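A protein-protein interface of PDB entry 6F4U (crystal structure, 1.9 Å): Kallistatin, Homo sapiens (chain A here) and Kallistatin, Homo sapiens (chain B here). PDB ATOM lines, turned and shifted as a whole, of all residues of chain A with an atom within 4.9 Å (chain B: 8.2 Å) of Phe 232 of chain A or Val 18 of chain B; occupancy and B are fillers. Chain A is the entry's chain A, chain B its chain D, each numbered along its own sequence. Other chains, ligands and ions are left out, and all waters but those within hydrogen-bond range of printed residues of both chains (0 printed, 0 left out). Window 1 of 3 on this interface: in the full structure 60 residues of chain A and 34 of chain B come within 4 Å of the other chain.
The backbone NH (N) of Leu 17 of chain B lies within hydrogen-bond range of the backbone carbonyl oxygen (O) of Ile 233 of chain A (2.8 Å). The backbone NH (N) of Phe 231 of chain A is in hydrogen-bond range of the backbone carbonyl oxygen (O) of Val 19 of chain B (2.9 Å).
The backbone carbonyl oxygen (O) of Ile 20 of chain B lies within hydrogen-bond range of the backbone NH (N) of Leu 29 of chain B, at 2.8 Å. The backbone NH of Val 18 of chain B is in hydrogen-bond range of the backbone carbonyl oxygen of Gly 32 of chain B, 2.9 Å away. O of Leu 220 of chain A sits at hydrogen-bond distance from N of Phe 232 of chain A. The backbone carbonyl oxygen of Val 230 of chain A sits at hydrogen-bond distance from the backbone NH of Met 222 of chain A (2.9 Å). The backbone NH (N) of Val 34 of chain B lies within hydrogen-bond range of the backbone carbonyl oxygen (O) of Phe 16 of chain B (2.8 Å). N of Leu 234 of chain A sits at hydrogen-bond distance from O of Ser 218 of chain A, at 2.8 Å.
Among the printed residues, pairs that only touch across the chains: Val 230 of chain A with Val 19 of chain B, Ile 233 of chain A with Phe 16 of chain B, Phe 232 of chain A with Leu 17 of chain B, Phe 30 of chain A with Phe 30 of chain B, Phe 231 of chain A with Val 18 of chain B, Phe 30 of chain A with Leu 31 of chain B, Phe 232 of chain A with Phe 12 of chain B, Phe 231 of chain A with Leu 17 of chain B, Ser 218 of chain A with Leu 10 of chain B, Leu 234 of chain A with Phe 12 of chain B, Leu 272 of chain A with Phe 12 of chain B, Val 230 of chain A with Val 18 of chain B, Val 230 of chain A with Ile 20 of chain B, Phe 232 of chain A with Phe 16 of chain B, Ile 233 of chain A with Val 19 of chain B, Leu 220 of chain A with Phe 12 of chain B, Phe 232 of chain A with Val 18 of chain B and Leu 220 of chain A with Leu 10 of chain B.
Of the printed residues of chain B, Leu 220 of chain A touches Leu 10 (3.99 Å) and Phe 12 (3.9 Å). Printed residues of chain B within 4 Å of Val 230 of chain A: Val 18 (3.8 Å), Val 19 (3.2 Å) and Ile 20 (3.9 Å). Phe 232 of chain A touches just these residues of chain B: Phe 12 (3.5 Å), Phe 16 (3.9 Å), Leu 17 (3.4 Å) and Val 18 (3.9 Å). Printed residues of chain B within 4 Å of Leu 234 of chain A: Phe 12 (3.7 Å). Leu 322 of chain A touches none of the printed residues of chain B. Of the printed residues of chain A, Phe 16 of chain B touches Phe 232 (3.9 Å) and Ile 233 (3.3 Å). Val 34 of chain B touches none of the printed residues of chain A. The nearest residue of chain B that does not touch Phe 232 of chain A is Val 19 of chain B (5.2 Å). The nearest residue of chain A that does not touch Val 18 of chain B is Leu 322 of chain A (4.3 Å).
Of the 16 printed residues of chain B, 9 touch a printed residue of chain A. Hydrophobic or aromatic side chains of chain B within 4 Å of the printed part of chain A: Leu 10, Phe 12, Phe 16, Leu 17, Val 18, Val 19, Ile 20 and Phe 30. Hydrophobic or aromatic side chains of chain A within 4 Å of the printed part of chain B: Phe 30, Leu 220, Val 230, Phe 231, Phe 232, Ile 233, Leu 234 and Leu 272. Along chain A the printed residues that touch a printed residue of chain B span positions 30 to 272. Among the printed residues, 20 pairs touch across the chains.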
ATOM      1  N   PHE A  30      17.761  35.401 -28.452  1.00  0.00           N
ATOM      2  CA  PHE A  30      17.545  35.285 -27.018  1.00  0.00           C
ATOM      3  C   PHE A  30      17.664  36.633 -26.316  1.00  0.00           C
ATOM      4  O   PHE A  30      18.683  37.302 -26.419  1.00  0.00           O
ATOM      5  CB  PHE A  30      18.476  34.228 -26.364  1.00  0.00           C
ATOM      6  CG  PHE A  30      18.024  33.821 -24.999  1.00  0.00           C
ATOM      7  CD1 PHE A  30      16.881  33.041 -24.838  1.00  0.00           C
ATOM      8  CD2 PHE A  30      18.705  34.240 -23.868  1.00  0.00           C
ATOM      9  CE1 PHE A  30      16.407  32.718 -23.580  1.00  0.00           C
ATOM     10  CE2 PHE A  30      18.224  33.932 -22.602  1.00  0.00           C
ATOM     11  CZ  PHE A  30      17.102  33.143 -22.450  1.00  0.00           C
ATOM     12  N   TRP A 173      14.719  21.873 -12.843  1.00  0.00           N
ATOM     13  CA  TRP A 173      13.528  21.233 -13.383  1.00  0.00           C
ATOM     14  C   TRP A 173      12.776  20.551 -12.251  1.00  0.00           C
ATOM     15  O   TRP A 173      13.390  19.954 -11.372  1.00  0.00           O
ATOM     16  CB  TRP A 173      13.859  20.149 -14.407  1.00  0.00           C
ATOM     17  CG  TRP A 173      14.618  20.563 -15.585  1.00  0.00           C
ATOM     18  CD1 TRP A 173      15.812  20.076 -15.983  1.00  0.00           C
ATOM     19  CD2 TRP A 173      14.210  21.509 -16.594  1.00  0.00           C
ATOM     20  NE1 TRP A 173      16.193  20.656 -17.159  1.00  0.00           N
ATOM     21  CE2 TRP A 173      15.240  21.567 -17.544  1.00  0.00           C
ATOM     22  CE3 TRP A 173      13.083  22.335 -16.763  1.00  0.00           C
ATOM     23  CZ2 TRP A 173      15.182  22.414 -18.672  1.00  0.00           C
ATOM     24  CZ3 TRP A 173      13.022  23.167 -17.880  1.00  0.00           C
ATOM     25  CH2 TRP A 173      14.059  23.200 -18.818  1.00  0.00           C
ATOM     26  N   SER A 218       3.702  21.619 -31.809  1.00  0.00           N
ATOM     27  CA  SER A 218       3.402  21.144 -30.476  1.00  0.00           C
ATOM     28  C   SER A 218       3.964  22.101 -29.429  1.00  0.00           C
ATOM     29  O   SER A 218       4.885  22.860 -29.712  1.00  0.00           O
ATOM     30  CB  SER A 218       4.024  19.764 -30.259  1.00  0.00           C
ATOM     31  OG  SER A 218       3.526  18.843 -31.230  1.00  0.00           O
ATOM     32  N   VAL A 219       3.415  22.022 -28.216  1.00  0.00           N
ATOM     33  CA  VAL A 219       3.769  22.900 -27.125  1.00  0.00           C
ATOM     34  C   VAL A 219       3.978  22.040 -25.888  1.00  0.00           C
ATOM     35  O   VAL A 219       3.124  21.231 -25.531  1.00  0.00           O
ATOM     36  CB  VAL A 219       2.691  23.978 -26.879  1.00  0.00           C
ATOM     37  CG1 VAL A 219       3.076  24.883 -25.713  1.00  0.00           C
ATOM     38  CG2 VAL A 219       2.450  24.805 -28.156  1.00  0.00           C
ATOM     39  N   LEU A 220       5.145  22.181 -25.277  1.00  0.00           N
ATOM     40  CA  LEU A 220       5.484  21.511 -24.019  1.00  0.00           C
ATOM     41  C   LEU A 220       5.669  22.594 -22.968  1.00  0.00           C
ATOM     42  O   LEU A 220       6.373  23.567 -23.223  1.00  0.00           O
ATOM     43  CB  LEU A 220       6.795  20.750 -24.180  1.00  0.00           C
ATOM     44  CG  LEU A 220       7.530  20.243 -22.921  1.00  0.00           C
ATOM     45  CD1 LEU A 220       6.705  19.224 -22.160  1.00  0.00           C
ATOM     46  CD2 LEU A 220       8.878  19.667 -23.336  1.00  0.00           C
ATOM     47  N   MET A 222       7.322  22.898 -19.272  1.00  0.00           N
ATOM     48  CA  MET A 222       8.079  22.257 -18.207  1.00  0.00           C
ATOM     49  C   MET A 222       8.112  23.174 -17.008  1.00  0.00           C
ATOM     50  O   MET A 222       8.419  24.367 -17.127  1.00  0.00           O
ATOM     51  CB  MET A 222       9.501  21.910 -18.658  1.00  0.00           C
ATOM     52  CG  MET A 222       9.532  20.813 -19.688  1.00  0.00           C
ATOM     53  SD  MET A 222      11.203  20.255 -20.097  1.00  0.00           S
ATOM     54  CE  MET A 222      11.692  19.458 -18.578  1.00  0.00           C
ATOM     55  N   VAL A 230       8.585  27.055 -18.315  1.00  0.00           N
ATOM     56  CA  VAL A 230       9.080  27.338 -19.639  1.00  0.00           C
ATOM     57  C   VAL A 230       8.188  26.634 -20.650  1.00  0.00           C
ATOM     58  O   VAL A 230       7.824  25.478 -20.464  1.00  0.00           O
ATOM     59  CB  VAL A 230      10.581  26.983 -19.805  1.00  0.00           C
ATOM     60  CG1 VAL A 230      10.876  25.516 -19.519  1.00  0.00           C
ATOM     61  CG2 VAL A 230      11.080  27.316 -21.207  1.00  0.00           C
ATOM     62  N   PHE A 231       7.814  27.364 -21.701  1.00  0.00           N
ATOM     63  CA  PHE A 231       7.146  26.777 -22.839  1.00  0.00           C
ATOM     64  C   PHE A 231       8.174  26.567 -23.922  1.00  0.00           C
ATOM     65  O   PHE A 231       8.845  27.519 -24.347  1.00  0.00           O
ATOM     66  CB  PHE A 231       6.062  27.717 -23.375  1.00  0.00           C
ATOM     67  CG  PHE A 231       4.987  27.993 -22.390  1.00  0.00           C
ATOM     68  CD1 PHE A 231       5.152  28.970 -21.422  1.00  0.00           C
ATOM     69  CD2 PHE A 231       3.827  27.271 -22.412  1.00  0.00           C
ATOM     70  CE1 PHE A 231       4.165  29.208 -20.473  1.00  0.00           C
ATOM     71  CE2 PHE A 231       2.815  27.524 -21.477  1.00  0.00           C
ATOM     72  CZ  PHE A 231       2.993  28.485 -20.510  1.00  0.00           C
ATOM     73  N   PHE A 232       8.278  25.322 -24.372  1.00  0.00           N
ATOM     74  CA  PHE A 232       9.060  24.954 -25.513  1.00  0.00           C
ATOM     75  C   PHE A 232       8.065  24.690 -26.650  1.00  0.00           C
ATOM     76  O   PHE A 232       7.229  23.778 -26.566  1.00  0.00           O
ATOM     77  CB  PHE A 232       9.891  23.698 -25.212  1.00  0.00           C
ATOM     78  CG  PHE A 232      11.064  23.922 -24.276  1.00  0.00           C
ATOM     79  CD1 PHE A 232      12.110  24.750 -24.633  1.00  0.00           C
ATOM     80  CD2 PHE A 232      11.137  23.261 -23.065  1.00  0.00           C
ATOM     81  CE1 PHE A 232      13.205  24.919 -23.797  1.00  0.00           C
ATOM     82  CE2 PHE A 232      12.216  23.432 -22.225  1.00  0.00           C
ATOM     83  CZ  PHE A 232      13.249  24.258 -22.595  1.00  0.00           C
ATOM     84  N   ILE A 233       8.124  25.518 -27.686  1.00  0.00           N
ATOM     85  CA  ILE A 233       7.179  25.443 -28.797  1.00  0.00           C
ATOM     86  C   ILE A 233       7.928  24.911 -30.014  1.00  0.00           C
ATOM     87  O   ILE A 233       8.946  25.466 -30.438  1.00  0.00           O
ATOM     88  CB  ILE A 233       6.550  26.806 -29.092  1.00  0.00           C
ATOM     89  CG1 ILE A 233       5.850  27.330 -27.833  1.00  0.00           C
ATOM     90  CG2 ILE A 233       5.573  26.714 -30.265  1.00  0.00           C
ATOM     91  CD1 ILE A 233       6.079  28.796 -27.621  1.00  0.00           C
ATOM     92  N   LEU A 234       7.419  23.804 -30.537  1.00  0.00           N
ATOM     93  CA  LEU A 234       8.091  23.027 -31.565  1.00  0.00           C
ATOM     94  C   LEU A 234       7.283  23.053 -32.842  1.00  0.00           C
ATOM     95  O   LEU A 234       6.332  22.270 -32.990  1.00  0.00           O
ATOM     96  CB  LEU A 234       8.274  21.587 -31.122  1.00  0.00           C
ATOM     97  CG  LEU A 234       9.054  20.656 -32.062  1.00  0.00           C
ATOM     98  CD1 LEU A 234      10.482  21.164 -32.275  1.00  0.00           C
ATOM     99  CD2 LEU A 234       9.068  19.272 -31.444  1.00  0.00           C
ATOM    100  N   LEU A 272      15.341  16.433 -25.660  1.00  0.00           N
ATOM    101  CA  LEU A 272      15.566  17.878 -25.572  1.00  0.00           C
ATOM    102  C   LEU A 272      17.065  18.103 -25.545  1.00  0.00           C
ATOM    103  O   LEU A 272      17.746  17.459 -24.743  1.00  0.00           O
ATOM    104  CB  LEU A 272      14.940  18.433 -24.292  1.00  0.00           C
ATOM    105  CG  LEU A 272      14.981  19.962 -24.096  1.00  0.00           C
ATOM    106  CD1 LEU A 272      14.051  20.610 -25.114  1.00  0.00           C
ATOM    107  CD2 LEU A 272      14.618  20.337 -22.649  1.00  0.00           C
ATOM    108  N   LEU A 322      21.357  31.783 -22.559  1.00  0.00           N
ATOM    109  CA  LEU A 322      20.532  30.635 -22.142  1.00  0.00           C
ATOM    110  C   LEU A 322      21.394  29.389 -22.078  1.00  0.00           C
ATOM    111  O   LEU A 322      22.071  29.093 -23.068  1.00  0.00           O
ATOM    112  CB  LEU A 322      19.437  30.376 -23.174  1.00  0.00           C
ATOM    113  CG  LEU A 322      18.478  29.207 -22.915  1.00  0.00           C
ATOM    114  CD1 LEU A 322      17.773  29.394 -21.586  1.00  0.00           C
ATOM    115  CD2 LEU A 322      17.478  29.085 -24.059  1.00  0.00           C
ATOM    116  N   VAL A 324      20.732  25.322 -21.002  1.00  0.00           N
ATOM    117  CA  VAL A 324      19.802  24.261 -20.672  1.00  0.00           C
ATOM    118  C   VAL A 324      20.604  22.958 -20.515  1.00  0.00           C
ATOM    119  O   VAL A 324      21.345  22.550 -21.419  1.00  0.00           O
ATOM    120  CB  VAL A 324      18.745  24.082 -21.777  1.00  0.00           C
ATOM    121  CG1 VAL A 324      17.961  22.787 -21.627  1.00  0.00           C
ATOM    122  CG2 VAL A 324      17.803  25.296 -21.794  1.00  0.00           C
ATOM    123  N   LEU B  10       8.023  13.792 -28.106  1.00  0.00           N
ATOM    124  CA  LEU B  10       8.481  15.047 -28.674  1.00  0.00           C
ATOM    125  C   LEU B  10       9.968  14.987 -28.829  1.00  0.00           C
ATOM    126  O   LEU B  10      10.670  14.644 -27.883  1.00  0.00           O
ATOM    127  CB  LEU B  10       8.099  16.246 -27.790  1.00  0.00           C
ATOM    128  CG  LEU B  10       6.612  16.596 -27.737  1.00  0.00           C
ATOM    129  CD1 LEU B  10       6.363  17.685 -26.705  1.00  0.00           C
ATOM    130  CD2 LEU B  10       6.092  17.036 -29.088  1.00  0.00           C
ATOM    131  N   PHE B  12      12.928  17.529 -29.841  1.00  0.00           N
ATOM    132  CA  PHE B  12      13.408  18.863 -30.147  1.00  0.00           C
ATOM    133  C   PHE B  12      14.718  18.794 -30.900  1.00  0.00           C
ATOM    134  O   PHE B  12      15.783  19.138 -30.373  1.00  0.00           O
ATOM    135  CB  PHE B  12      13.497  19.694 -28.867  1.00  0.00           C
ATOM    136  CG  PHE B  12      12.144  20.060 -28.315  1.00  0.00           C
ATOM    137  CD1 PHE B  12      11.426  19.168 -27.518  1.00  0.00           C
ATOM    138  CD2 PHE B  12      11.596  21.298 -28.583  1.00  0.00           C
ATOM    139  CE1 PHE B  12      10.174  19.517 -27.010  1.00  0.00           C
ATOM    140  CE2 PHE B  12      10.344  21.661 -28.082  1.00  0.00           C
ATOM    141  CZ  PHE B  12       9.625  20.751 -27.309  1.00  0.00           C
ATOM    142  N   PRO B  15      14.454  23.564 -35.215  1.00  0.00           N
ATOM    143  CA  PRO B  15      14.306  24.852 -34.516  1.00  0.00           C
ATOM    144  C   PRO B  15      13.060  24.956 -33.663  1.00  0.00           C
ATOM    145  O   PRO B  15      11.975  24.483 -34.056  1.00  0.00           O
ATOM    146  CB  PRO B  15      14.337  25.859 -35.655  1.00  0.00           C
ATOM    147  CG  PRO B  15      15.183  25.166 -36.692  1.00  0.00           C
ATOM    148  CD  PRO B  15      14.718  23.769 -36.647  1.00  0.00           C
ATOM    149  N   PHE B  16      13.214  25.558 -32.484  1.00  0.00           N
ATOM    150  CA  PHE B  16      12.112  25.681 -31.554  1.00  0.00           C
ATOM    151  C   PHE B  16      12.169  26.994 -30.792  1.00  0.00           C
ATOM    152  O   PHE B  16      13.206  27.673 -30.789  1.00  0.00           O
ATOM    153  CB  PHE B  16      12.079  24.459 -30.619  1.00  0.00           C
ATOM    154  CG  PHE B  16      13.308  24.304 -29.744  1.00  0.00           C
ATOM    155  CD1 PHE B  16      14.381  23.529 -30.163  1.00  0.00           C
ATOM    156  CD2 PHE B  16      13.380  24.887 -28.493  1.00  0.00           C
ATOM    157  CE1 PHE B  16      15.504  23.345 -29.365  1.00  0.00           C
ATOM    158  CE2 PHE B  16      14.501  24.693 -27.687  1.00  0.00           C
ATOM    159  CZ  PHE B  16      15.567  23.928 -28.127  1.00  0.00           C
ATOM    160  N   LEU B  17      11.046  27.362 -30.194  1.00  0.00           N
ATOM    161  CA  LEU B  17      10.927  28.592 -29.423  1.00  0.00           C
ATOM    162  C   LEU B  17      10.962  28.329 -27.935  1.00  0.00           C
ATOM    163  O   LEU B  17      10.568  27.252 -27.487  1.00  0.00           O
ATOM    164  CB  LEU B  17       9.638  29.340 -29.755  1.00  0.00           C
ATOM    165  CG  LEU B  17       9.463  29.666 -31.235  1.00  0.00           C
ATOM    166  CD1 LEU B  17       8.034  30.071 -31.527  1.00  0.00           C
ATOM    167  CD2 LEU B  17      10.425  30.748 -31.658  1.00  0.00           C
ATOM    168  N   VAL B  18      11.418  29.333 -27.180  1.00  0.00           N
ATOM    169  CA  VAL B  18      11.573  29.217 -25.744  1.00  0.00           C
ATOM    170  C   VAL B  18      10.930  30.437 -25.078  1.00  0.00           C
ATOM    171  O   VAL B  18      11.315  31.560 -25.386  1.00  0.00           O
ATOM    172  CB  VAL B  18      13.072  29.181 -25.361  1.00  0.00           C
ATOM    173  CG1 VAL B  18      13.226  29.094 -23.849  1.00  0.00           C
ATOM    174  CG2 VAL B  18      13.800  28.045 -26.051  1.00  0.00           C
ATOM    175  N   VAL B  19       9.986  30.202 -24.165  1.00  0.00           N
ATOM    176  CA  VAL B  19       9.332  31.273 -23.389  1.00  0.00           C
ATOM    177  C   VAL B  19       9.495  30.936 -21.897  1.00  0.00           C
ATOM    178  O   VAL B  19       8.848  30.030 -21.396  1.00  0.00           O
ATOM    179  CB  VAL B  19       7.834  31.424 -23.736  1.00  0.00           C
ATOM    180  CG1 VAL B  19       7.269  32.697 -23.106  1.00  0.00           C
ATOM    181  CG2 VAL B  19       7.628  31.460 -25.241  1.00  0.00           C
ATOM    182  N   ILE B  20      10.371  31.646 -21.205  1.00  0.00           N
ATOM    183  CA  ILE B  20      10.517  31.460 -19.749  1.00  0.00           C
ATOM    184  C   ILE B  20       9.623  32.485 -19.052  1.00  0.00           C
ATOM    185  O   ILE B  20       9.769  33.685 -19.265  1.00  0.00           O
ATOM    186  CB  ILE B  20      11.974  31.591 -19.303  1.00  0.00           C
ATOM    187  CG1 ILE B  20      12.825  30.533 -20.009  1.00  0.00           C
ATOM    188  CG2 ILE B  20      12.070  31.516 -17.770  1.00  0.00           C
ATOM    189  CD1 ILE B  20      14.312  30.657 -19.722  1.00  0.00           C
ATOM    190  N   PHE B  21       8.747  31.984 -18.187  1.00  0.00           N
ATOM    191  CA  PHE B  21       7.612  32.716 -17.660  1.00  0.00           C
ATOM    192  C   PHE B  21       7.569  32.646 -16.135  1.00  0.00           C
ATOM    193  O   PHE B  21       7.675  31.544 -15.580  1.00  0.00           O
ATOM    194  CB  PHE B  21       6.365  32.073 -18.287  1.00  0.00           C
ATOM    195  CG  PHE B  21       5.099  32.834 -18.056  1.00  0.00           C
ATOM    196  CD1 PHE B  21       4.087  32.294 -17.243  1.00  0.00           C
ATOM    197  CD2 PHE B  21       4.901  34.089 -18.640  1.00  0.00           C
ATOM    198  CE1 PHE B  21       2.884  32.992 -17.041  1.00  0.00           C
ATOM    199  CE2 PHE B  21       3.712  34.785 -18.428  1.00  0.00           C
ATOM    200  CZ  PHE B  21       2.706  34.231 -17.626  1.00  0.00           C
ATOM    201  N   VAL B  28       6.970  37.455 -18.863  1.00  0.00           N
ATOM    202  CA  VAL B  28       7.925  36.798 -19.742  1.00  0.00           C
ATOM    203  C   VAL B  28       9.307  37.295 -19.333  1.00  0.00           C
ATOM    204  O   VAL B  28       9.675  38.438 -19.578  1.00  0.00           O
ATOM    205  CB  VAL B  28       7.651  37.060 -21.230  1.00  0.00           C
ATOM    206  CG1 VAL B  28       8.685  36.329 -22.078  1.00  0.00           C
ATOM    207  CG2 VAL B  28       6.255  36.571 -21.620  1.00  0.00           C
ATOM    208  N   LEU B  29      10.072  36.421 -18.680  1.00  0.00           N
ATOM    209  CA  LEU B  29      11.417  36.746 -18.247  1.00  0.00           C
ATOM    210  C   LEU B  29      12.411  36.678 -19.392  1.00  0.00           C
ATOM    211  O   LEU B  29      13.329  37.513 -19.499  1.00  0.00           O
ATOM    212  CB  LEU B  29      11.854  35.807 -17.107  1.00  0.00           C
ATOM    213  CG  LEU B  29      10.991  35.761 -15.858  1.00  0.00           C
ATOM    214  CD1 LEU B  29      11.576  34.780 -14.844  1.00  0.00           C
ATOM    215  CD2 LEU B  29      10.804  37.140 -15.214  1.00  0.00           C
ATOM    216  N   PHE B  30      12.230  35.705 -20.273  1.00  0.00           N
ATOM    217  CA  PHE B  30      13.143  35.487 -21.401  1.00  0.00           C
ATOM    218  C   PHE B  30      12.354  34.904 -22.546  1.00  0.00           C
ATOM    219  O   PHE B  30      11.388  34.165 -22.346  1.00  0.00           O
ATOM    220  CB  PHE B  30      14.272  34.498 -21.048  1.00  0.00           C
ATOM    221  CG  PHE B  30      15.121  34.901 -19.887  1.00  0.00           C
ATOM    222  CD1 PHE B  30      16.260  35.676 -20.066  1.00  0.00           C
ATOM    223  CD2 PHE B  30      14.811  34.470 -18.596  1.00  0.00           C
ATOM    224  CE1 PHE B  30      17.051  36.032 -18.984  1.00  0.00           C
ATOM    225  CE2 PHE B  30      15.580  34.859 -17.506  1.00  0.00           C
ATOM    226  CZ  PHE B  30      16.712  35.618 -17.699  1.00  0.00           C
ATOM    227  N   LEU B  31      12.777  35.247 -23.761  1.00  0.00           N
ATOM    228  CA  LEU B  31      12.096  34.819 -24.958  1.00  0.00           C
ATOM    229  C   LEU B  31      13.166  34.556 -26.001  1.00  0.00           C
ATOM    230  O   LEU B  31      14.146  35.292 -26.090  1.00  0.00           O
ATOM    231  CB  LEU B  31      11.154  35.952 -25.387  1.00  0.00           C
ATOM    232  CG  LEU B  31      10.250  35.749 -26.571  1.00  0.00           C
ATOM    233  CD1 LEU B  31       9.453  34.453 -26.488  1.00  0.00           C
ATOM    234  CD2 LEU B  31       9.296  36.947 -26.653  1.00  0.00           C
ATOM    235  N   GLY B  32      13.022  33.489 -26.769  1.00  0.00           N
ATOM    236  CA  GLY B  32      13.990  33.267 -27.818  1.00  0.00           C
ATOM    237  C   GLY B  32      13.655  32.109 -28.724  1.00  0.00           C
ATOM    238  O   GLY B  32      12.590  31.527 -28.643  1.00  0.00           O
ATOM    239  N   LYS B  33      14.575  31.878 -29.638  1.00  0.00           N
ATOM    240  CA  LYS B  33      14.464  30.834 -30.627  1.00  0.00           C
ATOM    241  C   LYS B  33      15.819  30.165 -30.777  1.00  0.00           C
ATOM    242  O   LYS B  33      16.856  30.828 -30.950  1.00  0.00           O
ATOM    243  CB  LYS B  33      14.060  31.421 -31.970  1.00  0.00           C
ATOM    244  CG  LYS B  33      13.982  30.393 -33.092  1.00  0.00           C
ATOM    245  CD  LYS B  33      13.472  30.964 -34.402  1.00  0.00           C
ATOM    246  CE  LYS B  33      14.217  32.187 -34.861  1.00  0.00           C
ATOM    247  NZ  LYS B  33      13.640  32.593 -36.162  1.00  0.00           N
ATOM    248  N   VAL B  34      15.778  28.850 -30.780  1.00  0.00           N
ATOM    249  CA  VAL B  34      16.959  28.035 -31.061  1.00  0.00           C
ATOM    250  C   VAL B  34      16.870  27.553 -32.508  1.00  0.00           C
ATOM    251  O   VAL B  34      16.016  26.745 -32.832  1.00  0.00           O
ATOM    252  CB  VAL B  34      17.025  26.847 -30.068  1.00  0.00           C
ATOM    253  CG1 VAL B  34      18.199  25.939 -30.372  1.00  0.00           C
ATOM    254  CG2 VAL B  34      17.109  27.349 -28.610  1.00  0.00           C
